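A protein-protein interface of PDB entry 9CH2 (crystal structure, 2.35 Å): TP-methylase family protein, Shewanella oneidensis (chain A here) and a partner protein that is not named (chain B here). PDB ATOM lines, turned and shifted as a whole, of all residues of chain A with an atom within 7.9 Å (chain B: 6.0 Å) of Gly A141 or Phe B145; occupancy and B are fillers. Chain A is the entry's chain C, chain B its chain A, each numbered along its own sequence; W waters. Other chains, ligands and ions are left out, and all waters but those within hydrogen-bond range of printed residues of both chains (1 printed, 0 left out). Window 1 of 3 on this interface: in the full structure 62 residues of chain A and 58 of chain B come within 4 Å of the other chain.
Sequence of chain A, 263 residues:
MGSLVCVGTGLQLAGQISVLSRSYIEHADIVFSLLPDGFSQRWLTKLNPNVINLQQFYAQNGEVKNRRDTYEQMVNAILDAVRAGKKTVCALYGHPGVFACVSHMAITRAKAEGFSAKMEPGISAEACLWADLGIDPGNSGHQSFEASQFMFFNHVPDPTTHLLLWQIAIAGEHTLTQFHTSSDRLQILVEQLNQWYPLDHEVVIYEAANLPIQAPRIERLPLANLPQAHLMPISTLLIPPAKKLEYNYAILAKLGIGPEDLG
The backbone carbonyl oxygen (O) of His A142 is in hydrogen-bond range of the backbone NH (N) of Ser B144 (2.8 Å). N of Val B156 sits at hydrogen-bond distance from OD2 of Asp A158, 3.3 Å away. The side-chain amide nitrogen (NE2) of Gln B149 is in hydrogen-bond range of the backbone carbonyl oxygen (O) of Gly A138, at 3.2 Å. The backbone NH (N) of Phe B99 lies within hydrogen-bond range of the side-chain carboxylate (OD1) of Asp A136, 2.8 Å away. NE2 of Gln B149 lies within hydrogen-bond range of O of Asn A139 (2.6 Å). A ring nitrogen (ND1) of His B155 lies close to the side-chain hydroxyl of Thr A160 (3.1 Å). ND1 of His B155 lies within hydrogen-bond range of OD2 of Asp A158. OE1 of Gln B143 lies close to OE1 of Gln A143 (2.7 Å).
The backbone carbonyl oxygen (O) of Gln B143 sits at hydrogen-bond distance from the backbone NH (N) of Leu B164 (2.9 Å). The side-chain amide oxygen (OE1) of Gln B149 sits at hydrogen-bond distance from a ring nitrogen (NE2) of His B155, 2.7 Å away. OG of Ser A140 is in hydrogen-bond range of O of Thr A160. The backbone carbonyl oxygen (O) of Gly A141 lies within hydrogen-bond range of the backbone NH (N) of His A162. The backbone NH (N) of Phe B145 sits at hydrogen-bond distance from the backbone carbonyl oxygen (O) of Leu B164 (3.0 Å). OG1 of Thr A161 is in hydrogen-bond range of O of Asp A158.
Among the printed residues, merely in contact across the chains: Gly A138 with Phe B99, Ser A140 with Gln B149, Ser A140 with His B155, Gly A141 with Ser B144, Gly A141 with Phe B145, Gly A141 with Gln B149, His A142 with Gln B143, Gln A143 with Val B156, Asp A158 with Phe B145, Thr A161 with Phe B145, Leu A245 with Gln B149 and Leu A245 with His B155.
Of the printed residues of chain B, Asn A139 touches Gln B149. Of chain B, only Ser B144, Phe B145 and Gln B149 come within 4 Å of Gly A141. Printed residues of chain B within 4 Å of His A142: Gln B143 (3.2 Å) and Ser B144 (2.8 Å). Phe B145 touches three residues of chain A. Ala B147 touches none of the printed residues of chain A. Of the printed residues of chain A, His B155 touches Ser A140, Asp A158, Thr A160 and Leu A245. Pro B157 touches none of the printed residues of chain A. The nearest residue of chain B that does not touch Gly A141 is His B155 (4.8 Å). The nearest printed residue of chain A that does not touch His B155 is Thr A161 (4.03 Å).
Hydrophobic or aromatic side chains of chain A within 4 Å of the printed part of chain B: Leu A245. Among the printed residues, no Asp or Glu carboxylate lies within 4 Å of a Lys or Arg side-chain nitrogen of the other chain.
Water W1 lies within hydrogen-bond range of the backbone carbonyl oxygen (O) of Gly A138 (2.6 Å), the backbone NH (N) of Glu B146 (2.9 Å), the side-chain amide oxygen (OE1) of Gln B149 (3.0 Å) and the backbone NH (N) of Gly A141 (3.4 Å).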
ATOM      1  N   TRP A 130     -26.669  28.836 -34.813  1.00  0.00           N
ATOM      2  CA  TRP A 130     -27.791  28.762 -33.891  1.00  0.00           C
ATOM      3  C   TRP A 130     -28.840  29.807 -34.258  1.00  0.00           C
ATOM      4  O   TRP A 130     -30.035  29.521 -34.270  1.00  0.00           O
ATOM      5  CB  TRP A 130     -27.312  28.958 -32.445  1.00  0.00           C
ATOM      6  CG  TRP A 130     -26.317  27.932 -31.971  1.00  0.00           C
ATOM      7  CD1 TRP A 130     -25.211  28.166 -31.208  1.00  0.00           C
ATOM      8  CD2 TRP A 130     -26.344  26.507 -32.210  1.00  0.00           C
ATOM      9  NE1 TRP A 130     -24.542  26.997 -30.965  1.00  0.00           N
ATOM     10  CE2 TRP A 130     -25.212  25.963 -31.563  1.00  0.00           C
ATOM     11  CE3 TRP A 130     -27.201  25.645 -32.902  1.00  0.00           C
ATOM     12  CZ2 TRP A 130     -24.923  24.601 -31.592  1.00  0.00           C
ATOM     13  CZ3 TRP A 130     -26.914  24.298 -32.927  1.00  0.00           C
ATOM     14  CH2 TRP A 130     -25.790  23.785 -32.281  1.00  0.00           C
ATOM     15  N   ILE A 135     -31.975  27.367 -33.817  1.00  0.00           N
ATOM     16  CA  ILE A 135     -31.832  26.144 -33.047  1.00  0.00           C
ATOM     17  C   ILE A 135     -31.087  26.462 -31.753  1.00  0.00           C
ATOM     18  O   ILE A 135     -30.063  27.142 -31.772  1.00  0.00           O
ATOM     19  CB  ILE A 135     -31.105  25.065 -33.870  1.00  0.00           C
ATOM     20  CG1 ILE A 135     -31.898  24.682 -35.118  1.00  0.00           C
ATOM     21  CG2 ILE A 135     -30.783  23.845 -33.006  1.00  0.00           C
ATOM     22  CD1 ILE A 135     -31.142  23.789 -36.084  1.00  0.00           C
ATOM     23  N   ASP A 136     -31.619  25.960 -30.634  1.00  0.00           N
ATOM     24  CA  ASP A 136     -30.982  26.127 -29.340  1.00  0.00           C
ATOM     25  C   ASP A 136     -30.201  24.859 -29.009  1.00  0.00           C
ATOM     26  O   ASP A 136     -30.782  23.782 -28.892  1.00  0.00           O
ATOM     27  CB  ASP A 136     -31.995  26.453 -28.255  1.00  0.00           C
ATOM     28  CG  ASP A 136     -31.401  26.959 -26.949  1.00  0.00           C
ATOM     29  OD1 ASP A 136     -30.412  26.355 -26.484  1.00  0.00           O
ATOM     30  OD2 ASP A 136     -31.936  27.948 -26.405  1.00  0.00           O
ATOM     31  N   PRO A 137     -28.862  24.946 -28.845  1.00  0.00           N
ATOM     32  CA  PRO A 137     -28.051  23.771 -28.525  1.00  0.00           C
ATOM     33  C   PRO A 137     -28.511  23.107 -27.230  1.00  0.00           C
ATOM     34  O   PRO A 137     -28.276  21.920 -27.017  1.00  0.00           O
ATOM     35  CB  PRO A 137     -26.616  24.324 -28.430  1.00  0.00           C
ATOM     36  CG  PRO A 137     -26.793  25.815 -28.213  1.00  0.00           C
ATOM     37  CD  PRO A 137     -28.069  26.179 -28.950  1.00  0.00           C
ATOM     38  N   GLY A 138     -29.177  23.891 -26.375  1.00  0.00           N
ATOM     39  CA  GLY A 138     -29.663  23.399 -25.097  1.00  0.00           C
ATOM     40  C   GLY A 138     -30.938  22.579 -25.263  1.00  0.00           C
ATOM     41  O   GLY A 138     -31.275  21.766 -24.405  1.00  0.00           O
ATOM     42  N   ASN A 139     -31.637  22.801 -26.381  1.00  0.00           N
ATOM     43  CA  ASN A 139     -32.909  22.147 -26.640  1.00  0.00           C
ATOM     44  C   ASN A 139     -32.788  20.657 -26.333  1.00  0.00           C
ATOM     45  O   ASN A 139     -33.482  20.141 -25.459  1.00  0.00           O
ATOM     46  CB  ASN A 139     -33.380  22.383 -28.071  1.00  0.00           C
ATOM     47  CG  ASN A 139     -34.777  21.858 -28.304  1.00  0.00           C
ATOM     48  OD1 ASN A 139     -34.965  20.904 -29.066  1.00  0.00           O
ATOM     49  ND2 ASN A 139     -35.763  22.457 -27.654  1.00  0.00           N
ATOM     50  N   SER A 140     -31.903  19.973 -27.066  1.00  0.00           N
ATOM     51  CA  SER A 140     -31.702  18.545 -26.885  1.00  0.00           C
ATOM     52  C   SER A 140     -30.212  18.234 -26.778  1.00  0.00           C
ATOM     53  O   SER A 140     -29.800  17.086 -26.935  1.00  0.00           O
ATOM     54  CB  SER A 140     -32.348  17.759 -28.001  1.00  0.00           C
ATOM     55  OG  SER A 140     -31.783  18.093 -29.262  1.00  0.00           O
ATOM     56  N   GLY A 141     -29.411  19.268 -26.502  1.00  0.00           N
ATOM     57  CA  GLY A 141     -27.972  19.111 -26.375  1.00  0.00           C
ATOM     58  C   GLY A 141     -27.277  19.302 -27.721  1.00  0.00           C
ATOM     59  O   GLY A 141     -27.934  19.491 -28.743  1.00  0.00           O
ATOM     60  N   HIS A 142     -25.943  19.234 -27.706  1.00  0.00           N
ATOM     61  CA  HIS A 142     -25.151  19.549 -28.884  1.00  0.00           C
ATOM     62  C   HIS A 142     -23.750  18.957 -28.755  1.00  0.00           C
ATOM     63  O   HIS A 142     -23.114  19.067 -27.709  1.00  0.00           O
ATOM     64  CB  HIS A 142     -25.153  21.064 -29.117  1.00  0.00           C
ATOM     65  CG  HIS A 142     -23.848  21.622 -29.577  1.00  0.00           C
ATOM     66  ND1 HIS A 142     -23.088  22.446 -28.776  1.00  0.00           N
ATOM     67  CD2 HIS A 142     -23.186  21.517 -30.736  1.00  0.00           C
ATOM     68  CE1 HIS A 142     -21.995  22.804 -29.433  1.00  0.00           C
ATOM     69  NE2 HIS A 142     -22.033  22.251 -30.624  1.00  0.00           N
ATOM     70  N   GLN A 143     -23.289  18.325 -29.841  1.00  0.00           N
ATOM     71  CA  GLN A 143     -21.935  17.805 -29.926  1.00  0.00           C
ATOM     72  C   GLN A 143     -21.276  18.337 -31.197  1.00  0.00           C
ATOM     73  O   GLN A 143     -21.892  18.347 -32.260  1.00  0.00           O
ATOM     74  CB  GLN A 143     -21.932  16.277 -29.942  1.00  0.00           C
ATOM     75  CG  GLN A 143     -22.617  15.641 -28.737  1.00  0.00           C
ATOM     76  CD  GLN A 143     -22.479  14.134 -28.703  1.00  0.00           C
ATOM     77  OE1 GLN A 143     -21.950  13.556 -27.747  1.00  0.00           O
ATOM     78  NE2 GLN A 143     -22.958  13.483 -29.751  1.00  0.00           N
ATOM     79  N   ASP A 158     -24.319  11.053 -29.735  1.00  0.00           N
ATOM     80  CA  ASP A 158     -25.624  10.897 -29.115  1.00  0.00           C
ATOM     81  C   ASP A 158     -26.681  11.441 -30.071  1.00  0.00           C
ATOM     82  O   ASP A 158     -26.846  12.653 -30.195  1.00  0.00           O
ATOM     83  CB  ASP A 158     -25.675  11.587 -27.761  1.00  0.00           C
ATOM     84  CG  ASP A 158     -27.054  11.667 -27.125  1.00  0.00           C
ATOM     85  OD1 ASP A 158     -28.012  11.147 -27.736  1.00  0.00           O
ATOM     86  OD2 ASP A 158     -27.160  12.254 -26.027  1.00  0.00           O
ATOM     87  N   THR A 160     -29.628  12.126 -30.085  1.00  0.00           N
ATOM     88  CA  THR A 160     -30.713  12.948 -29.574  1.00  0.00           C
ATOM     89  C   THR A 160     -30.313  14.419 -29.670  1.00  0.00           C
ATOM     90  O   THR A 160     -31.165  15.302 -29.601  1.00  0.00           O
ATOM     91  CB  THR A 160     -31.055  12.561 -28.135  1.00  0.00           C
ATOM     92  OG1 THR A 160     -29.869  12.786 -27.378  1.00  0.00           O
ATOM     93  CG2 THR A 160     -31.508  11.118 -28.009  1.00  0.00           C
ATOM     94  N   THR A 161     -29.008  14.667 -29.834  1.00  0.00           N
ATOM     95  CA  THR A 161     -28.478  16.020 -29.861  1.00  0.00           C
ATOM     96  C   THR A 161     -28.401  16.512 -31.303  1.00  0.00           C
ATOM     97  O   THR A 161     -28.623  15.749 -32.241  1.00  0.00           O
ATOM     98  CB  THR A 161     -27.095  16.046 -29.210  1.00  0.00           C
ATOM     99  OG1 THR A 161     -26.247  15.340 -30.112  1.00  0.00           O
ATOM    100  CG2 THR A 161     -27.075  15.395 -27.839  1.00  0.00           C
ATOM    101  N   HIS A 162     -28.084  17.802 -31.455  1.00  0.00           N
ATOM    102  CA  HIS A 162     -27.667  18.352 -32.733  1.00  0.00           C
ATOM    103  C   HIS A 162     -26.164  18.132 -32.879  1.00  0.00           C
ATOM    104  O   HIS A 162     -25.380  18.612 -32.061  1.00  0.00           O
ATOM    105  CB  HIS A 162     -28.047  19.834 -32.840  1.00  0.00           C
ATOM    106  CG  HIS A 162     -29.494  20.080 -33.120  1.00  0.00           C
ATOM    107  ND1 HIS A 162     -30.437  20.260 -32.131  1.00  0.00           N
ATOM    108  CD2 HIS A 162     -30.153  20.187 -34.283  1.00  0.00           C
ATOM    109  CE1 HIS A 162     -31.624  20.462 -32.689  1.00  0.00           C
ATOM    110  NE2 HIS A 162     -31.474  20.422 -33.995  1.00  0.00           N
ATOM    111  N   LEU A 163     -25.775  17.391 -33.921  1.00  0.00           N
ATOM    112  CA  LEU A 163     -24.385  17.020 -34.129  1.00  0.00           C
ATOM    113  C   LEU A 163     -23.784  17.883 -35.236  1.00  0.00           C
ATOM    114  O   LEU A 163     -24.364  18.013 -36.312  1.00  0.00           O
ATOM    115  CB  LEU A 163     -24.300  15.534 -34.474  1.00  0.00           C
ATOM    116  CG  LEU A 163     -22.918  15.020 -34.891  1.00  0.00           C
ATOM    117  CD1 LEU A 163     -21.935  15.071 -33.734  1.00  0.00           C
ATOM    118  CD2 LEU A 163     -23.018  13.611 -35.449  1.00  0.00           C
ATOM    119  N   PRO A 241     -31.192  15.737 -34.653  1.00  0.00           N
ATOM    120  CA  PRO A 241     -31.506  14.490 -33.953  1.00  0.00           C
ATOM    121  C   PRO A 241     -32.221  13.483 -34.849  1.00  0.00           C
ATOM    122  O   PRO A 241     -33.003  13.865 -35.717  1.00  0.00           O
ATOM    123  CB  PRO A 241     -32.396  14.955 -32.784  1.00  0.00           C
ATOM    124  CG  PRO A 241     -31.995  16.396 -32.555  1.00  0.00           C
ATOM    125  CD  PRO A 241     -31.665  16.932 -33.937  1.00  0.00           C
ATOM    126  N   LEU A 245     -35.767  12.502 -27.244  1.00  0.00           N
ATOM    127  CA  LEU A 245     -35.386  12.298 -25.858  1.00  0.00           C
ATOM    128  C   LEU A 245     -36.310  11.268 -25.216  1.00  0.00           C
ATOM    129  O   LEU A 245     -37.503  11.229 -25.510  1.00  0.00           O
ATOM    130  CB  LEU A 245     -35.452  13.635 -25.121  1.00  0.00           C
ATOM    131  CG  LEU A 245     -34.404  14.679 -25.519  1.00  0.00           C
ATOM    132  CD1 LEU A 245     -34.788  16.052 -24.998  1.00  0.00           C
ATOM    133  CD2 LEU A 245     -33.029  14.283 -25.012  1.00  0.00           C
ATOM    134  N   PHE B  99     -29.369  28.435 -24.901  1.00  0.00           N
ATOM    135  CA  PHE B  99     -29.986  28.143 -23.617  1.00  0.00           C
ATOM    136  C   PHE B  99     -30.864  29.322 -23.204  1.00  0.00           C
ATOM    137  O   PHE B  99     -30.707  29.868 -22.115  1.00  0.00           O
ATOM    138  CB  PHE B  99     -28.908  27.828 -22.575  1.00  0.00           C
ATOM    139  CG  PHE B  99     -28.162  26.520 -22.806  1.00  0.00           C
ATOM    140  CD1 PHE B  99     -27.057  26.465 -23.648  1.00  0.00           C
ATOM    141  CD2 PHE B  99     -28.565  25.347 -22.175  1.00  0.00           C
ATOM    142  CE1 PHE B  99     -26.380  25.272 -23.854  1.00  0.00           C
ATOM    143  CE2 PHE B  99     -27.885  24.158 -22.385  1.00  0.00           C
ATOM    144  CZ  PHE B  99     -26.794  24.123 -23.223  1.00  0.00           C
ATOM    145  N   GLN B 143     -18.997  19.355 -26.278  1.00  0.00           N
ATOM    146  CA  GLN B 143     -20.382  18.960 -26.086  1.00  0.00           C
ATOM    147  C   GLN B 143     -21.026  19.890 -25.062  1.00  0.00           C
ATOM    148  O   GLN B 143     -20.337  20.440 -24.206  1.00  0.00           O
ATOM    149  CB  GLN B 143     -20.473  17.539 -25.528  1.00  0.00           C
ATOM    150  CG  GLN B 143     -19.728  16.489 -26.342  1.00  0.00           C
ATOM    151  CD  GLN B 143     -19.543  15.194 -25.582  1.00  0.00           C
ATOM    152  OE1 GLN B 143     -20.170  14.171 -25.882  1.00  0.00           O
ATOM    153  NE2 GLN B 143     -18.690  15.233 -24.569  1.00  0.00           N
ATOM    154  N   SER B 144     -22.353  20.039 -25.142  1.00  0.00           N
ATOM    155  CA  SER B 144     -23.085  20.859 -24.192  1.00  0.00           C
ATOM    156  C   SER B 144     -24.452  20.244 -23.904  1.00  0.00           C
ATOM    157  O   SER B 144     -25.159  19.823 -24.818  1.00  0.00           O
ATOM    158  CB  SER B 144     -23.219  22.280 -24.682  1.00  0.00           C
ATOM    159  OG  SER B 144     -21.951  22.918 -24.745  1.00  0.00           O
ATOM    160  N   PHE B 145     -24.805  20.200 -22.615  1.00  0.00           N
ATOM    161  CA  PHE B 145     -26.109  19.730 -22.181  1.00  0.00           C
ATOM    162  C   PHE B 145     -26.590  20.600 -21.025  1.00  0.00           C
ATOM    163  O   PHE B 145     -25.784  21.125 -20.259  1.00  0.00           O
ATOM    164  CB  PHE B 145     -26.079  18.270 -21.720  1.00  0.00           C
ATOM    165  CG  PHE B 145     -25.629  17.258 -22.765  1.00  0.00           C
ATOM    166  CD1 PHE B 145     -26.542  16.689 -23.646  1.00  0.00           C
ATOM    167  CD2 PHE B 145     -24.300  16.861 -22.847  1.00  0.00           C
ATOM    168  CE1 PHE B 145     -26.131  15.761 -24.590  1.00  0.00           C
ATOM    169  CE2 PHE B 145     -23.895  15.932 -23.792  1.00  0.00           C
ATOM    170  CZ  PHE B 145     -24.811  15.385 -24.660  1.00  0.00           C
ATOM    171  N   GLU B 146     -27.914  20.737 -20.911  1.00  0.00           N
ATOM    172  CA  GLU B 146     -28.524  21.362 -19.750  1.00  0.00           C
ATOM    173  C   GLU B 146     -28.506  20.341 -18.614  1.00  0.00           C
ATOM    174  O   GLU B 146     -29.037  19.242 -18.753  1.00  0.00           O
ATOM    175  CB  GLU B 146     -29.922  21.856 -20.127  1.00  0.00           C
ATOM    176  CG  GLU B 146     -30.508  22.868 -19.148  1.00  0.00           C
ATOM    177  CD  GLU B 146     -31.168  22.267 -17.920  1.00  0.00           C
ATOM    178  OE1 GLU B 146     -31.299  21.027 -17.865  1.00  0.00           O
ATOM    179  OE2 GLU B 146     -31.551  23.043 -17.018  1.00  0.00           O
ATOM    180  N   ALA B 147     -27.866  20.714 -17.501  1.00  0.00           N
ATOM    181  CA  ALA B 147     -27.578  19.783 -16.420  1.00  0.00           C
ATOM    182  C   ALA B 147     -28.809  18.941 -16.092  1.00  0.00           C
ATOM    183  O   ALA B 147     -28.711  17.724 -15.954  1.00  0.00           O
ATOM    184  CB  ALA B 147     -27.089  20.542 -15.207  1.00  0.00           C
ATOM    185  N   GLN B 149     -31.490  18.352 -17.918  1.00  0.00           N
ATOM    186  CA  GLN B 149     -31.879  17.509 -19.036  1.00  0.00           C
ATOM    187  C   GLN B 149     -30.987  16.270 -19.059  1.00  0.00           C
ATOM    188  O   GLN B 149     -31.436  15.184 -19.416  1.00  0.00           O
ATOM    189  CB  GLN B 149     -31.791  18.258 -20.366  1.00  0.00           C
ATOM    190  CG  GLN B 149     -32.304  17.453 -21.556  1.00  0.00           C
ATOM    191  CD  GLN B 149     -32.062  18.129 -22.888  1.00  0.00           C
ATOM    192  OE1 GLN B 149     -31.297  17.643 -23.728  1.00  0.00           O
ATOM    193  NE2 GLN B 149     -32.711  19.266 -23.092  1.00  0.00           N
ATOM    194  N   PHE B 150     -29.721  16.453 -18.670  1.00  0.00           N
ATOM    195  CA  PHE B 150     -28.748  15.373 -18.678  1.00  0.00           C
ATOM    196  C   PHE B 150     -29.137  14.337 -17.627  1.00  0.00           C
ATOM    197  O   PHE B 150     -28.824  13.158 -17.767  1.00  0.00           O
ATOM    198  CB  PHE B 150     -27.339  15.918 -18.429  1.00  0.00           C
ATOM    199  CG  PHE B 150     -26.233  14.877 -18.545  1.00  0.00           C
ATOM    200  CD1 PHE B 150     -25.639  14.604 -19.773  1.00  0.00           C
ATOM    201  CD2 PHE B 150     -25.793  14.174 -17.431  1.00  0.00           C
ATOM    202  CE1 PHE B 150     -24.634  13.655 -19.878  1.00  0.00           C
ATOM    203  CE2 PHE B 150     -24.787  13.226 -17.541  1.00  0.00           C
ATOM    204  CZ  PHE B 150     -24.211  12.969 -18.764  1.00  0.00           C
ATOM    205  N   HIS B 155     -28.986  10.771 -22.023  1.00  0.00           N
ATOM    206  CA  HIS B 155     -27.914  11.318 -22.836  1.00  0.00           C
ATOM    207  C   HIS B 155     -26.648  10.503 -22.589  1.00  0.00           C
ATOM    208  O   HIS B 155     -26.416  10.031 -21.479  1.00  0.00           O
ATOM    209  CB  HIS B 155     -27.700  12.804 -22.524  1.00  0.00           C
ATOM    210  CG  HIS B 155     -28.637  13.717 -23.243  1.00  0.00           C
ATOM    211  ND1 HIS B 155     -28.906  13.598 -24.589  1.00  0.00           N
ATOM    212  CD2 HIS B 155     -29.340  14.773 -22.815  1.00  0.00           C
ATOM    213  CE1 HIS B 155     -29.758  14.548 -24.949  1.00  0.00           C
ATOM    214  NE2 HIS B 155     -30.035  15.272 -23.886  1.00  0.00           N
ATOM    215  N   VAL B 156     -25.842  10.339 -23.642  1.00  0.00           N
ATOM    216  CA  VAL B 156     -24.581   9.627 -23.536  1.00  0.00           C
ATOM    217  C   VAL B 156     -23.462  10.563 -23.981  1.00  0.00           C
ATOM    218  O   VAL B 156     -23.349  10.886 -25.160  1.00  0.00           O
ATOM    219  CB  VAL B 156     -24.573   8.328 -24.364  1.00  0.00           C
ATOM    220  CG1 VAL B 156     -23.227   7.617 -24.280  1.00  0.00           C
ATOM    221  CG2 VAL B 156     -25.703   7.391 -23.958  1.00  0.00           C
ATOM    222  N   PRO B 157     -22.604  11.028 -23.047  1.00  0.00           N
ATOM    223  CA  PRO B 157     -21.485  11.897 -23.404  1.00  0.00           C
ATOM    224  C   PRO B 157     -20.344  11.103 -24.034  1.00  0.00           C
ATOM    225  O   PRO B 157     -20.220   9.903 -23.804  1.00  0.00           O
ATOM    226  CB  PRO B 157     -21.101  12.506 -22.047  1.00  0.00           C
ATOM    227  CG  PRO B 157     -21.418  11.408 -21.057  1.00  0.00           C
ATOM    228  CD  PRO B 157     -22.670  10.738 -21.606  1.00  0.00           C
ATOM    229  N   LEU B 163     -16.823  18.376 -22.060  1.00  0.00           N
ATOM    230  CA  LEU B 163     -18.247  18.305 -21.779  1.00  0.00           C
ATOM    231  C   LEU B 163     -18.646  19.482 -20.893  1.00  0.00           C
ATOM    232  O   LEU B 163     -18.068  19.685 -19.827  1.00  0.00           O
ATOM    233  CB  LEU B 163     -18.563  16.966 -21.112  1.00  0.00           C
ATOM    234  CG  LEU B 163     -19.947  16.846 -20.465  1.00  0.00           C
ATOM    235  CD1 LEU B 163     -21.053  17.037 -21.486  1.00  0.00           C
ATOM    236  CD2 LEU B 163     -20.098  15.510 -19.757  1.00  0.00           C
ATOM    237  N   LEU B 164     -19.640  20.251 -21.352  1.00  0.00           N
ATOM    238  CA  LEU B 164     -20.157  21.380 -20.596  1.00  0.00           C
ATOM    239  C   LEU B 164     -21.571  21.064 -20.119  1.00  0.00           C
ATOM    240  O   LEU B 164     -22.431  20.695 -20.916  1.00  0.00           O
ATOM    241  CB  LEU B 164     -20.145  22.644 -21.454  1.00  0.00           C
ATOM    242  CG  LEU B 164     -18.769  23.171 -21.874  1.00  0.00           C
ATOM    243  CD1 LEU B 164     -18.921  24.394 -22.761  1.00  0.00           C
ATOM    244  CD2 LEU B 164     -17.912  23.493 -20.664  1.00  0.00           C
ATOM    245  N   LEU B 165     -21.799  21.227 -18.811  1.00  0.00           N
ATOM    246  CA  LEU B 165     -23.131  21.117 -18.239  1.00  0.00           C
ATOM    247  C   LEU B 165     -23.582  22.499 -17.778  1.00  0.00           C
ATOM    248  O   LEU B 165     -23.014  23.056 -16.840  1.00  0.00           O
ATOM    249  CB  LEU B 165     -23.137  20.117 -17.083  1.00  0.00           C
ATOM    250  CG  LEU B 165     -22.811  18.665 -17.441  1.00  0.00           C
ATOM    251  CD1 LEU B 165     -22.979  17.771 -16.225  1.00  0.00           C
ATOM    252  CD2 LEU B 165     -23.669  18.171 -18.593  1.00  0.00           C
ATOM    253  N   TRP B 166     -24.613  23.038 -18.441  1.00  0.00           N
ATOM    254  CA  TRP B 166     -25.105  24.374 -18.148  1.00  0.00           C
ATOM    255  C   TRP B 166     -26.136  24.326 -17.022  1.00  0.00           C
ATOM    256  O   TRP B 166     -26.734  23.286 -16.760  1.00  0.00           O
ATOM    257  CB  TRP B 166     -25.710  25.019 -19.403  1.00  0.00           C
ATOM    258  CG  TRP B 166     -24.734  25.223 -20.532  1.00  0.00           C
ATOM    259  CD1 TRP B 166     -23.883  24.301 -21.068  1.00  0.00           C
ATOM    260  CD2 TRP B 166     -24.503  26.451 -21.255  1.00  0.00           C
ATOM    261  NE1 TRP B 166     -23.150  24.862 -22.079  1.00  0.00           N
ATOM    262  CE2 TRP B 166     -23.504  26.179 -22.216  1.00  0.00           C
ATOM    263  CE3 TRP B 166     -25.039  27.742 -21.188  1.00  0.00           C
ATOM    264  CZ2 TRP B 166     -23.038  27.152 -23.097  1.00  0.00           C
ATOM    265  CZ3 TRP B 166     -24.574  28.703 -22.058  1.00  0.00           C
ATOM    266  CH2 TRP B 166     -23.587  28.410 -22.998  1.00  0.00           C
ATOM    267  N   GLN B 167     -26.330  25.477 -16.365  1.00  0.00           N
ATOM    268  CA  GLN B 167     -27.331  25.623 -15.322  1.00  0.00           C
ATOM    269  C   GLN B 167     -27.157  24.507 -14.295  1.00  0.00           C
ATOM    270  O   GLN B 167     -28.114  23.824 -13.939  1.00  0.00           O
ATOM    271  CB  GLN B 167     -28.727  25.620 -15.948  1.00  0.00           C
ATOM    272  CG  GLN B 167     -28.912  26.677 -17.033  1.00  0.00           C
ATOM    273  CD  GLN B 167     -30.305  26.696 -17.623  1.00  0.00           C
ATOM    274  OE1 GLN B 167     -31.180  25.907 -17.247  1.00  0.00           O
ATOM    275  NE2 GLN B 167     -30.524  27.605 -18.561  1.00  0.00           N
HETATM  276  O   HOH W   1     -29.595  20.109 -23.236  1.00  0.00           O
